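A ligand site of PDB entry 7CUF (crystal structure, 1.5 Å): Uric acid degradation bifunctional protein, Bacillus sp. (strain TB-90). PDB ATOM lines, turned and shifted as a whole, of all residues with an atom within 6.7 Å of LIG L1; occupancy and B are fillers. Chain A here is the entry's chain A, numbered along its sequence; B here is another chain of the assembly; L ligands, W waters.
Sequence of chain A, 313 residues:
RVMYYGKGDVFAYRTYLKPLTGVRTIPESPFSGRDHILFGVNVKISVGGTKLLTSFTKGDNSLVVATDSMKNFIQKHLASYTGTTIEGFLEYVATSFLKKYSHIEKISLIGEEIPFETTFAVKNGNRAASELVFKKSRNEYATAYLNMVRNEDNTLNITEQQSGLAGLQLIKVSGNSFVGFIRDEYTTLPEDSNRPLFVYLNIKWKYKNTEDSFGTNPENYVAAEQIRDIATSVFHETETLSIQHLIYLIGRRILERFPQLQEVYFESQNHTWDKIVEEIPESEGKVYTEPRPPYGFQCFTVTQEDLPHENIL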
ATOM      1  N   SER A 177     -29.437 -21.179  17.882  1.00  0.00           N
ATOM      2  CA  SER A 177     -28.963 -19.813  18.038  1.00  0.00           C
ATOM      3  C   SER A 177     -28.465 -19.597  19.462  1.00  0.00           C
ATOM      4  O   SER A 177     -28.806 -20.335  20.402  1.00  0.00           O
ATOM      5  CB  SER A 177     -30.056 -18.781  17.731  1.00  0.00           C
ATOM      6  OG  SER A 177     -30.994 -18.621  18.766  1.00  0.00           O
ATOM      7  N   PHE A 178     -27.616 -18.576  19.607  1.00  0.00           N
ATOM      8  CA  PHE A 178     -27.297 -18.016  20.931  1.00  0.00           C
ATOM      9  C   PHE A 178     -27.210 -16.504  20.744  1.00  0.00           C
ATOM     10  O   PHE A 178     -26.194 -15.982  20.267  1.00  0.00           O
ATOM     11  CB  PHE A 178     -26.039 -18.604  21.532  1.00  0.00           C
ATOM     12  CG  PHE A 178     -25.819 -18.201  22.970  1.00  0.00           C
ATOM     13  CD1 PHE A 178     -26.787 -18.435  23.936  1.00  0.00           C
ATOM     14  CD2 PHE A 178     -24.673 -17.538  23.356  1.00  0.00           C
ATOM     15  CE1 PHE A 178     -26.607 -18.037  25.266  1.00  0.00           C
ATOM     16  CE2 PHE A 178     -24.486 -17.137  24.674  1.00  0.00           C
ATOM     17  CZ  PHE A 178     -25.437 -17.403  25.617  1.00  0.00           C
ATOM     18  N   PHE A 181     -27.777 -12.309  24.796  1.00  0.00           N
ATOM     19  CA  PHE A 181     -27.058 -12.370  26.066  1.00  0.00           C
ATOM     20  C   PHE A 181     -26.441 -10.991  26.402  1.00  0.00           C
ATOM     21  O   PHE A 181     -26.390 -10.076  25.576  1.00  0.00           O
ATOM     22  CB  PHE A 181     -26.036 -13.504  26.057  1.00  0.00           C
ATOM     23  CG  PHE A 181     -25.096 -13.464  24.904  1.00  0.00           C
ATOM     24  CD1 PHE A 181     -23.917 -12.725  24.967  1.00  0.00           C
ATOM     25  CD2 PHE A 181     -25.388 -14.156  23.723  1.00  0.00           C
ATOM     26  CE1 PHE A 181     -23.045 -12.683  23.875  1.00  0.00           C
ATOM     27  CE2 PHE A 181     -24.492 -14.150  22.637  1.00  0.00           C
ATOM     28  CZ  PHE A 181     -23.330 -13.372  22.699  1.00  0.00           C
ATOM     29  N   LEU A 189     -18.050 -12.205  22.706  1.00  0.00           N
ATOM     30  CA  LEU A 189     -18.676 -13.274  21.935  1.00  0.00           C
ATOM     31  C   LEU A 189     -19.660 -12.659  20.941  1.00  0.00           C
ATOM     32  O   LEU A 189     -20.571 -11.945  21.368  1.00  0.00           O
ATOM     33  CB  LEU A 189     -19.444 -14.209  22.888  1.00  0.00           C
ATOM     34  CG  LEU A 189     -20.124 -15.422  22.252  1.00  0.00           C
ATOM     35  CD1 LEU A 189     -19.066 -16.293  21.606  1.00  0.00           C
ATOM     36  CD2 LEU A 189     -20.952 -16.219  23.294  1.00  0.00           C
ATOM     37  N   ARG A 195     -25.611 -21.704  14.844  1.00  0.00           N
ATOM     38  CA  ARG A 195     -24.349 -22.320  15.215  1.00  0.00           C
ATOM     39  C   ARG A 195     -24.472 -23.837  15.196  1.00  0.00           C
ATOM     40  O   ARG A 195     -25.573 -24.382  15.341  1.00  0.00           O
ATOM     41  CB  ARG A 195     -23.892 -21.883  16.608  1.00  0.00           C
ATOM     42  CG  ARG A 195     -24.928 -22.114  17.669  1.00  0.00           C
ATOM     43  CD  ARG A 195     -24.353 -21.757  19.003  1.00  0.00           C
ATOM     44  NE  ARG A 195     -25.230 -22.165  20.082  1.00  0.00           N
ATOM     45  CZ  ARG A 195     -24.977 -21.998  21.366  1.00  0.00           C
ATOM     46  NH1 ARG A 195     -23.829 -21.450  21.751  1.00  0.00           N
ATOM     47  NH2 ARG A 195     -25.845 -22.405  22.284  1.00  0.00           N
ATOM     48  N   LEU A 197     -24.240 -26.404  17.323  1.00  0.00           N
ATOM     49  CA  LEU A 197     -24.108 -26.612  18.749  1.00  0.00           C
ATOM     50  C   LEU A 197     -23.605 -28.022  19.031  1.00  0.00           C
ATOM     51  O   LEU A 197     -24.191 -29.012  18.562  1.00  0.00           O
ATOM     52  CB  LEU A 197     -25.454 -26.371  19.420  1.00  0.00           C
ATOM     53  CG  LEU A 197     -25.479 -26.608  20.940  1.00  0.00           C
ATOM     54  CD1 LEU A 197     -24.447 -25.785  21.682  1.00  0.00           C
ATOM     55  CD2 LEU A 197     -26.874 -26.238  21.429  1.00  0.00           C
ATOM     56  N   LEU A 241     -32.205 -22.263  21.674  1.00  0.00           N
ATOM     57  CA  LEU A 241     -31.865 -20.868  21.968  1.00  0.00           C
ATOM     58  C   LEU A 241     -30.686 -20.726  22.912  1.00  0.00           C
ATOM     59  O   LEU A 241     -30.262 -19.596  23.185  1.00  0.00           O
ATOM     60  CB  LEU A 241     -33.091 -20.151  22.563  1.00  0.00           C
ATOM     61  CG  LEU A 241     -34.353 -20.104  21.689  1.00  0.00           C
ATOM     62  CD1 LEU A 241     -35.557 -19.650  22.503  1.00  0.00           C
ATOM     63  CD2 LEU A 241     -34.134 -19.170  20.515  1.00  0.00           C
ATOM     64  N   SER A 242     -30.193 -21.855  23.472  1.00  0.00           N
ATOM     65  CA  SER A 242     -29.070 -21.955  24.394  1.00  0.00           C
ATOM     66  C   SER A 242     -29.040 -23.432  24.783  1.00  0.00           C
ATOM     67  O   SER A 242     -30.035 -24.140  24.584  1.00  0.00           O
ATOM     68  CB  SER A 242     -29.251 -21.130  25.644  1.00  0.00           C
ATOM     69  OG  SER A 242     -30.331 -21.604  26.404  1.00  0.00           O
ATOM     70  N   ILE A 243     -27.925 -23.892  25.356  1.00  0.00           N
ATOM     71  CA  ILE A 243     -27.928 -25.216  25.971  1.00  0.00           C
ATOM     72  C   ILE A 243     -28.921 -25.279  27.122  1.00  0.00           C
ATOM     73  O   ILE A 243     -29.603 -26.302  27.317  1.00  0.00           O
ATOM     74  CB  ILE A 243     -26.518 -25.602  26.408  1.00  0.00           C
ATOM     75  CG1 ILE A 243     -25.591 -25.802  25.207  1.00  0.00           C
ATOM     76  CG2 ILE A 243     -26.551 -26.928  27.181  1.00  0.00           C
ATOM     77  CD1 ILE A 243     -24.099 -25.697  25.615  1.00  0.00           C
ATOM     78  N   GLN A 244     -29.028 -24.209  27.897  1.00  0.00           N
ATOM     79  CA  GLN A 244     -29.969 -24.172  29.001  1.00  0.00           C
ATOM     80  C   GLN A 244     -31.388 -24.502  28.525  1.00  0.00           C
ATOM     81  O   GLN A 244     -32.077 -25.333  29.129  1.00  0.00           O
ATOM     82  CB  GLN A 244     -29.930 -22.770  29.647  1.00  0.00           C
ATOM     83  CG  GLN A 244     -28.623 -22.443  30.434  1.00  0.00           C
ATOM     84  CD  GLN A 244     -27.549 -21.734  29.583  1.00  0.00           C
ATOM     85  OE1 GLN A 244     -27.313 -22.091  28.433  1.00  0.00           O
ATOM     86  NE2 GLN A 244     -26.881 -20.751  30.182  1.00  0.00           N
ATOM     87  N   ASN A 270     -20.477 -27.208  26.703  1.00  0.00           N
ATOM     88  CA  ASN A 270     -20.476 -26.654  25.344  1.00  0.00           C
ATOM     89  C   ASN A 270     -19.085 -26.827  24.732  1.00  0.00           C
ATOM     90  O   ASN A 270     -18.099 -26.300  25.268  1.00  0.00           O
ATOM     91  CB  ASN A 270     -20.781 -25.155  25.409  1.00  0.00           C
ATOM     92  CG  ASN A 270     -21.089 -24.566  24.061  1.00  0.00           C
ATOM     93  OD1 ASN A 270     -20.774 -25.149  23.020  1.00  0.00           O
ATOM     94  ND2 ASN A 270     -21.701 -23.398  24.076  1.00  0.00           N
ATOM     95  N   GLY A 296     -17.969 -23.901  28.362  1.00  0.00           N
ATOM     96  CA  GLY A 296     -19.114 -23.552  29.177  1.00  0.00           C
ATOM     97  C   GLY A 296     -19.780 -24.799  29.722  1.00  0.00           C
ATOM     98  O   GLY A 296     -19.691 -25.904  29.146  1.00  0.00           O
ATOM     99  N   PHE A 297     -20.483 -24.673  30.837  1.00  0.00           N
ATOM    100  CA  PHE A 297     -21.215 -25.803  31.362  1.00  0.00           C
ATOM    101  C   PHE A 297     -22.467 -25.289  32.036  1.00  0.00           C
ATOM    102  O   PHE A 297     -22.562 -24.122  32.431  1.00  0.00           O
ATOM    103  CB  PHE A 297     -20.356 -26.699  32.309  1.00  0.00           C
ATOM    104  CG  PHE A 297     -19.910 -26.000  33.565  1.00  0.00           C
ATOM    105  CD1 PHE A 297     -20.752 -25.889  34.644  1.00  0.00           C
ATOM    106  CD2 PHE A 297     -18.654 -25.465  33.651  1.00  0.00           C
ATOM    107  CE1 PHE A 297     -20.313 -25.225  35.820  1.00  0.00           C
ATOM    108  CE2 PHE A 297     -18.237 -24.804  34.805  1.00  0.00           C
ATOM    109  CZ  PHE A 297     -19.077 -24.670  35.866  1.00  0.00           C
ATOM    110  N   GLN A 298     -23.425 -26.212  32.168  1.00  0.00           N
ATOM    111  CA  GLN A 298     -24.721 -25.950  32.773  1.00  0.00           C
ATOM    112  C   GLN A 298     -25.107 -27.144  33.629  1.00  0.00           C
ATOM    113  O   GLN A 298     -24.772 -28.287  33.323  1.00  0.00           O
ATOM    114  CB  GLN A 298     -25.797 -25.764  31.707  1.00  0.00           C
ATOM    115  CG  GLN A 298     -25.578 -24.639  30.745  1.00  0.00           C
ATOM    116  CD  GLN A 298     -24.524 -24.895  29.680  1.00  0.00           C
ATOM    117  OE1 GLN A 298     -24.241 -26.032  29.295  1.00  0.00           O
ATOM    118  NE2 GLN A 298     -23.937 -23.797  29.179  1.00  0.00           N
ATOM    119  N   TYR B   5     -24.558 -22.423  36.160  1.00  0.00           N
ATOM    120  CA  TYR B   5     -23.793 -22.595  34.912  1.00  0.00           C
ATOM    121  C   TYR B   5     -22.480 -21.840  35.092  1.00  0.00           C
ATOM    122  O   TYR B   5     -22.289 -21.097  36.066  1.00  0.00           O
ATOM    123  CB  TYR B   5     -24.639 -22.148  33.700  1.00  0.00           C
ATOM    124  CG  TYR B   5     -24.669 -20.666  33.495  1.00  0.00           C
ATOM    125  CD1 TYR B   5     -25.225 -19.790  34.446  1.00  0.00           C
ATOM    126  CD2 TYR B   5     -24.158 -20.129  32.332  1.00  0.00           C
ATOM    127  CE1 TYR B   5     -25.254 -18.424  34.240  1.00  0.00           C
ATOM    128  CE2 TYR B   5     -24.173 -18.756  32.102  1.00  0.00           C
ATOM    129  CZ  TYR B   5     -24.703 -17.908  33.053  1.00  0.00           C
ATOM    130  OH  TYR B   5     -24.698 -16.558  32.846  1.00  0.00           O
ATOM    131  N   GLY B   6     -21.535 -22.094  34.182  1.00  0.00           N
ATOM    132  CA  GLY B   6     -20.238 -21.456  34.291  1.00  0.00           C
ATOM    133  C   GLY B   6     -19.260 -21.885  33.225  1.00  0.00           C
ATOM    134  O   GLY B   6     -19.638 -22.272  32.116  1.00  0.00           O
ATOM    135  N   LYS B   7     -18.004 -21.762  33.566  1.00  0.00           N
ATOM    136  CA  LYS B   7     -16.930 -22.006  32.633  1.00  0.00           C
ATOM    137  C   LYS B   7     -15.844 -22.831  33.320  1.00  0.00           C
ATOM    138  O   LYS B   7     -15.429 -22.504  34.436  1.00  0.00           O
ATOM    139  CB  LYS B   7     -16.338 -20.680  32.180  1.00  0.00           C
ATOM    140  CG  LYS B   7     -15.496 -20.795  30.915  1.00  0.00           C
ATOM    141  CD  LYS B   7     -16.393 -20.882  29.681  1.00  0.00           C
ATOM    142  CE  LYS B   7     -15.656 -20.581  28.386  1.00  0.00           C
ATOM    143  NZ  LYS B   7     -16.605 -20.634  27.221  1.00  0.00           N
ATOM    144  N   ASN B  61     -32.272 -15.104  27.186  1.00  0.00           N
ATOM    145  CA  ASN B  61     -30.876 -14.851  27.482  1.00  0.00           C
ATOM    146  C   ASN B  61     -30.633 -13.446  28.039  1.00  0.00           C
ATOM    147  O   ASN B  61     -29.470 -13.111  28.299  1.00  0.00           O
ATOM    148  CB  ASN B  61     -30.013 -15.111  26.245  1.00  0.00           C
ATOM    149  CG  ASN B  61     -29.958 -16.588  25.888  1.00  0.00           C
ATOM    150  OD1 ASN B  61     -29.943 -17.441  26.784  1.00  0.00           O
ATOM    151  ND2 ASN B  61     -29.936 -16.903  24.605  1.00  0.00           N
ATOM    152  N   VAL B  64     -28.308 -13.583  30.963  1.00  0.00           N
ATOM    153  CA  VAL B  64     -27.213 -14.526  30.816  1.00  0.00           C
ATOM    154  C   VAL B  64     -25.923 -13.769  30.540  1.00  0.00           C
ATOM    155  O   VAL B  64     -25.764 -13.160  29.479  1.00  0.00           O
ATOM    156  CB  VAL B  64     -27.499 -15.576  29.731  1.00  0.00           C
ATOM    157  CG1 VAL B  64     -26.304 -16.505  29.563  1.00  0.00           C
ATOM    158  CG2 VAL B  64     -28.729 -16.396  30.113  1.00  0.00           C
ATOM    159  N   VAL B  65     -25.002 -13.833  31.485  1.00  0.00           N
ATOM    160  CA  VAL B  65     -23.603 -13.515  31.210  1.00  0.00           C
ATOM    161  C   VAL B  65     -23.038 -14.685  30.405  1.00  0.00           C
ATOM    162  O   VAL B  65     -23.026 -15.828  30.879  1.00  0.00           O
ATOM    163  CB  VAL B  65     -22.835 -13.337  32.515  1.00  0.00           C
ATOM    164  CG1 VAL B  65     -21.370 -13.074  32.258  1.00  0.00           C
ATOM    165  CG2 VAL B  65     -23.403 -12.213  33.375  1.00  0.00           C
ATOM    166  N   ALA B  66     -22.602 -14.429  29.198  1.00  0.00           N
ATOM    167  CA  ALA B  66     -22.043 -15.524  28.407  1.00  0.00           C
ATOM    168  C   ALA B  66     -20.879 -16.174  29.164  1.00  0.00           C
ATOM    169  O   ALA B  66     -20.081 -15.518  29.830  1.00  0.00           O
ATOM    170  CB  ALA B  66     -21.615 -15.028  27.034  1.00  0.00           C
ATOM    171  N   THR B  67     -20.791 -17.491  29.065  1.00  0.00           N
ATOM    172  CA  THR B  67     -19.651 -18.138  29.725  1.00  0.00           C
ATOM    173  C   THR B  67     -18.327 -17.636  29.157  1.00  0.00           C
ATOM    174  O   THR B  67     -17.323 -17.530  29.890  1.00  0.00           O
ATOM    175  CB  THR B  67     -19.761 -19.650  29.665  1.00  0.00           C
ATOM    176  OG1 THR B  67     -19.609 -20.134  28.326  1.00  0.00           O
ATOM    177  CG2 THR B  67     -21.098 -20.127  30.198  1.00  0.00           C
ATOM    178  N   ASP B  68     -18.313 -17.298  27.847  1.00  0.00           N
ATOM    179  CA  ASP B  68     -17.129 -16.705  27.252  1.00  0.00           C
ATOM    180  C   ASP B  68     -16.745 -15.427  27.971  1.00  0.00           C
ATOM    181  O   ASP B  68     -15.547 -15.125  28.127  1.00  0.00           O
ATOM    182  CB  ASP B  68     -17.398 -16.373  25.774  1.00  0.00           C
ATOM    183  CG  ASP B  68     -16.153 -15.886  25.047  1.00  0.00           C
ATOM    184  OD1 ASP B  68     -15.333 -16.739  24.676  1.00  0.00           O
ATOM    185  OD2 ASP B  68     -15.996 -14.654  24.851  1.00  0.00           O
ATOM    186  N   SER B  69     -17.736 -14.656  28.399  1.00  0.00           N
ATOM    187  CA  SER B  69     -17.435 -13.422  29.117  1.00  0.00           C
ATOM    188  C   SER B  69     -16.877 -13.691  30.495  1.00  0.00           C
ATOM    189  O   SER B  69     -16.051 -12.912  30.963  1.00  0.00           O
ATOM    190  CB  SER B  69     -18.693 -12.577  29.187  1.00  0.00           C
ATOM    191  OG  SER B  69     -19.228 -12.452  27.872  1.00  0.00           O
ATOM    192  N   MET B  70     -17.335 -14.766  31.169  1.00  0.00           N
ATOM    193  CA  MET B  70     -16.731 -15.218  32.414  1.00  0.00           C
ATOM    194  C   MET B  70     -15.245 -15.509  32.249  1.00  0.00           C
ATOM    195  O   MET B  70     -14.438 -15.161  33.123  1.00  0.00           O
ATOM    196  CB  MET B  70     -17.457 -16.471  32.881  1.00  0.00           C
ATOM    197  CG  MET B  70     -18.879 -16.234  33.197  1.00  0.00           C
ATOM    198  SD  MET B  70     -19.699 -17.686  33.855  1.00  0.00           S
ATOM    199  CE  MET B  70     -21.371 -17.306  33.480  1.00  0.00           C
HETATM  200  N1  LIG L   1     -25.115 -21.041  26.901  1.00  0.00           N
HETATM  201  C1  LIG L   1     -24.953 -21.442  25.604  1.00  0.00           C
HETATM  202  O1  LIG L   1     -25.716 -22.225  25.122  1.00  0.00           O
HETATM  203  N2  LIG L   1     -23.942 -20.952  24.858  1.00  0.00           N
HETATM  204  C2  LIG L   1     -23.103 -20.080  25.397  1.00  0.00           C
HETATM  205  C3  LIG L   1     -23.230 -19.687  26.704  1.00  0.00           C
HETATM  206  C4  LIG L   1     -24.282 -20.172  27.469  1.00  0.00           C
HETATM  207  O2  LIG L   1     -24.463 -19.891  28.610  1.00  0.00           O
HETATM  208  N3  LIG L   1     -22.223 -18.803  26.918  1.00  0.00           N
HETATM  209  N4  LIG L   1     -21.480 -18.703  25.805  1.00  0.00           N
HETATM  210  N5  LIG L   1     -22.033 -19.504  24.864  1.00  0.00           N
HETATM  211  O1  LG2 L   2     -21.056 -22.000  26.885  1.00  0.00           O
HETATM  212  O2  LG2 L   2     -22.028 -22.525  27.412  1.00  0.00           O
HETATM  213  O   HOH W   1     -20.919 -19.907  22.445  1.00  0.00           O
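The backbone NH (N) of Ile 243 is in hydrogen-bond range of an oxygen (O1) of LIG L1.
The guanidinium group (NH2) of Arg 195 sits at hydrogen-bond distance from an oxygen (O1) of LIG L1, 2.8 Å away.
A nitrogen (N1) of LIG L1 sits at hydrogen-bond distance from the side-chain amide oxygen (OE1) of Gln 244 (2.9 Å).
The backbone NH (N) of Thr 67 of chain B is in hydrogen-bond range of a nitrogen (N3) of LIG L1.
A nitrogen (N3) of LIG L1 lies within hydrogen-bond range of the side-chain hydroxyl (OG1) of Thr 67 of chain B (3.3 Å).
The side-chain amide nitrogen of Asn 270 sits close to a nitrogen (N2) of LIG L1 (3.4 Å).
An oxygen (O1) of LG2 L2 is in hydrogen-bond range of the side-chain hydroxyl (OG1) of Thr 67 of chain B (2.8 Å).
ND2 of Asn 270 lies within hydrogen-bond range of O1 of LG2 L2 (3.2 Å).
NE2 of Gln 298 is in hydrogen-bond range of O2 of LG2 L2 (2.9 Å).
An oxygen (O2) of LG2 L2 lies close to a nitrogen (N1) of LIG L1.
The side-chain hydroxyl (OG) of Ser 242 lies close to the backbone NH (N) of Gln 244, 3.3 Å away.
The side-chain hydroxyl (OG1) of Thr 67 of chain B lies within hydrogen-bond range of the side-chain amino group (NZ) of Lys 7 of chain B (3.2 Å).
The backbone NH (N) of Asn 270 sits at hydrogen-bond distance from the backbone carbonyl oxygen (O) of Gly 296 (2.9 Å).
The backbone carbonyl oxygen of Val 65 of chain B lies within hydrogen-bond range of the side-chain hydroxyl of Tyr 5 of chain B, at 2.7 Å.
Merely in contact with LIG L1: Phe 178, Ser 242, Leu 189, Ala 66 of chain B, Tyr 5 of chain B, Gln 298 and Val 64 of chain B.
Hydrophobic or aromatic side chains within 4 Å of LIG L1: Phe 178, Leu 189, Ile 243, Tyr 5 of chain B, Val 64 of chain B and Ala 66 of chain B.
Within 4 Å of LIG L1: Phe 178, Leu 189, Arg 195, Ser 242, Ile 243, Gln 244, Asn 270, Gln 298, Tyr 5 of chain B, Val 64 of chain B, Ala 66 of chain B and Thr 67 of chain B.
Water W1 lies within hydrogen-bond range of N5 of LIG L1 (2.7 Å) and NH1 of Arg 195 (3.4 Å).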
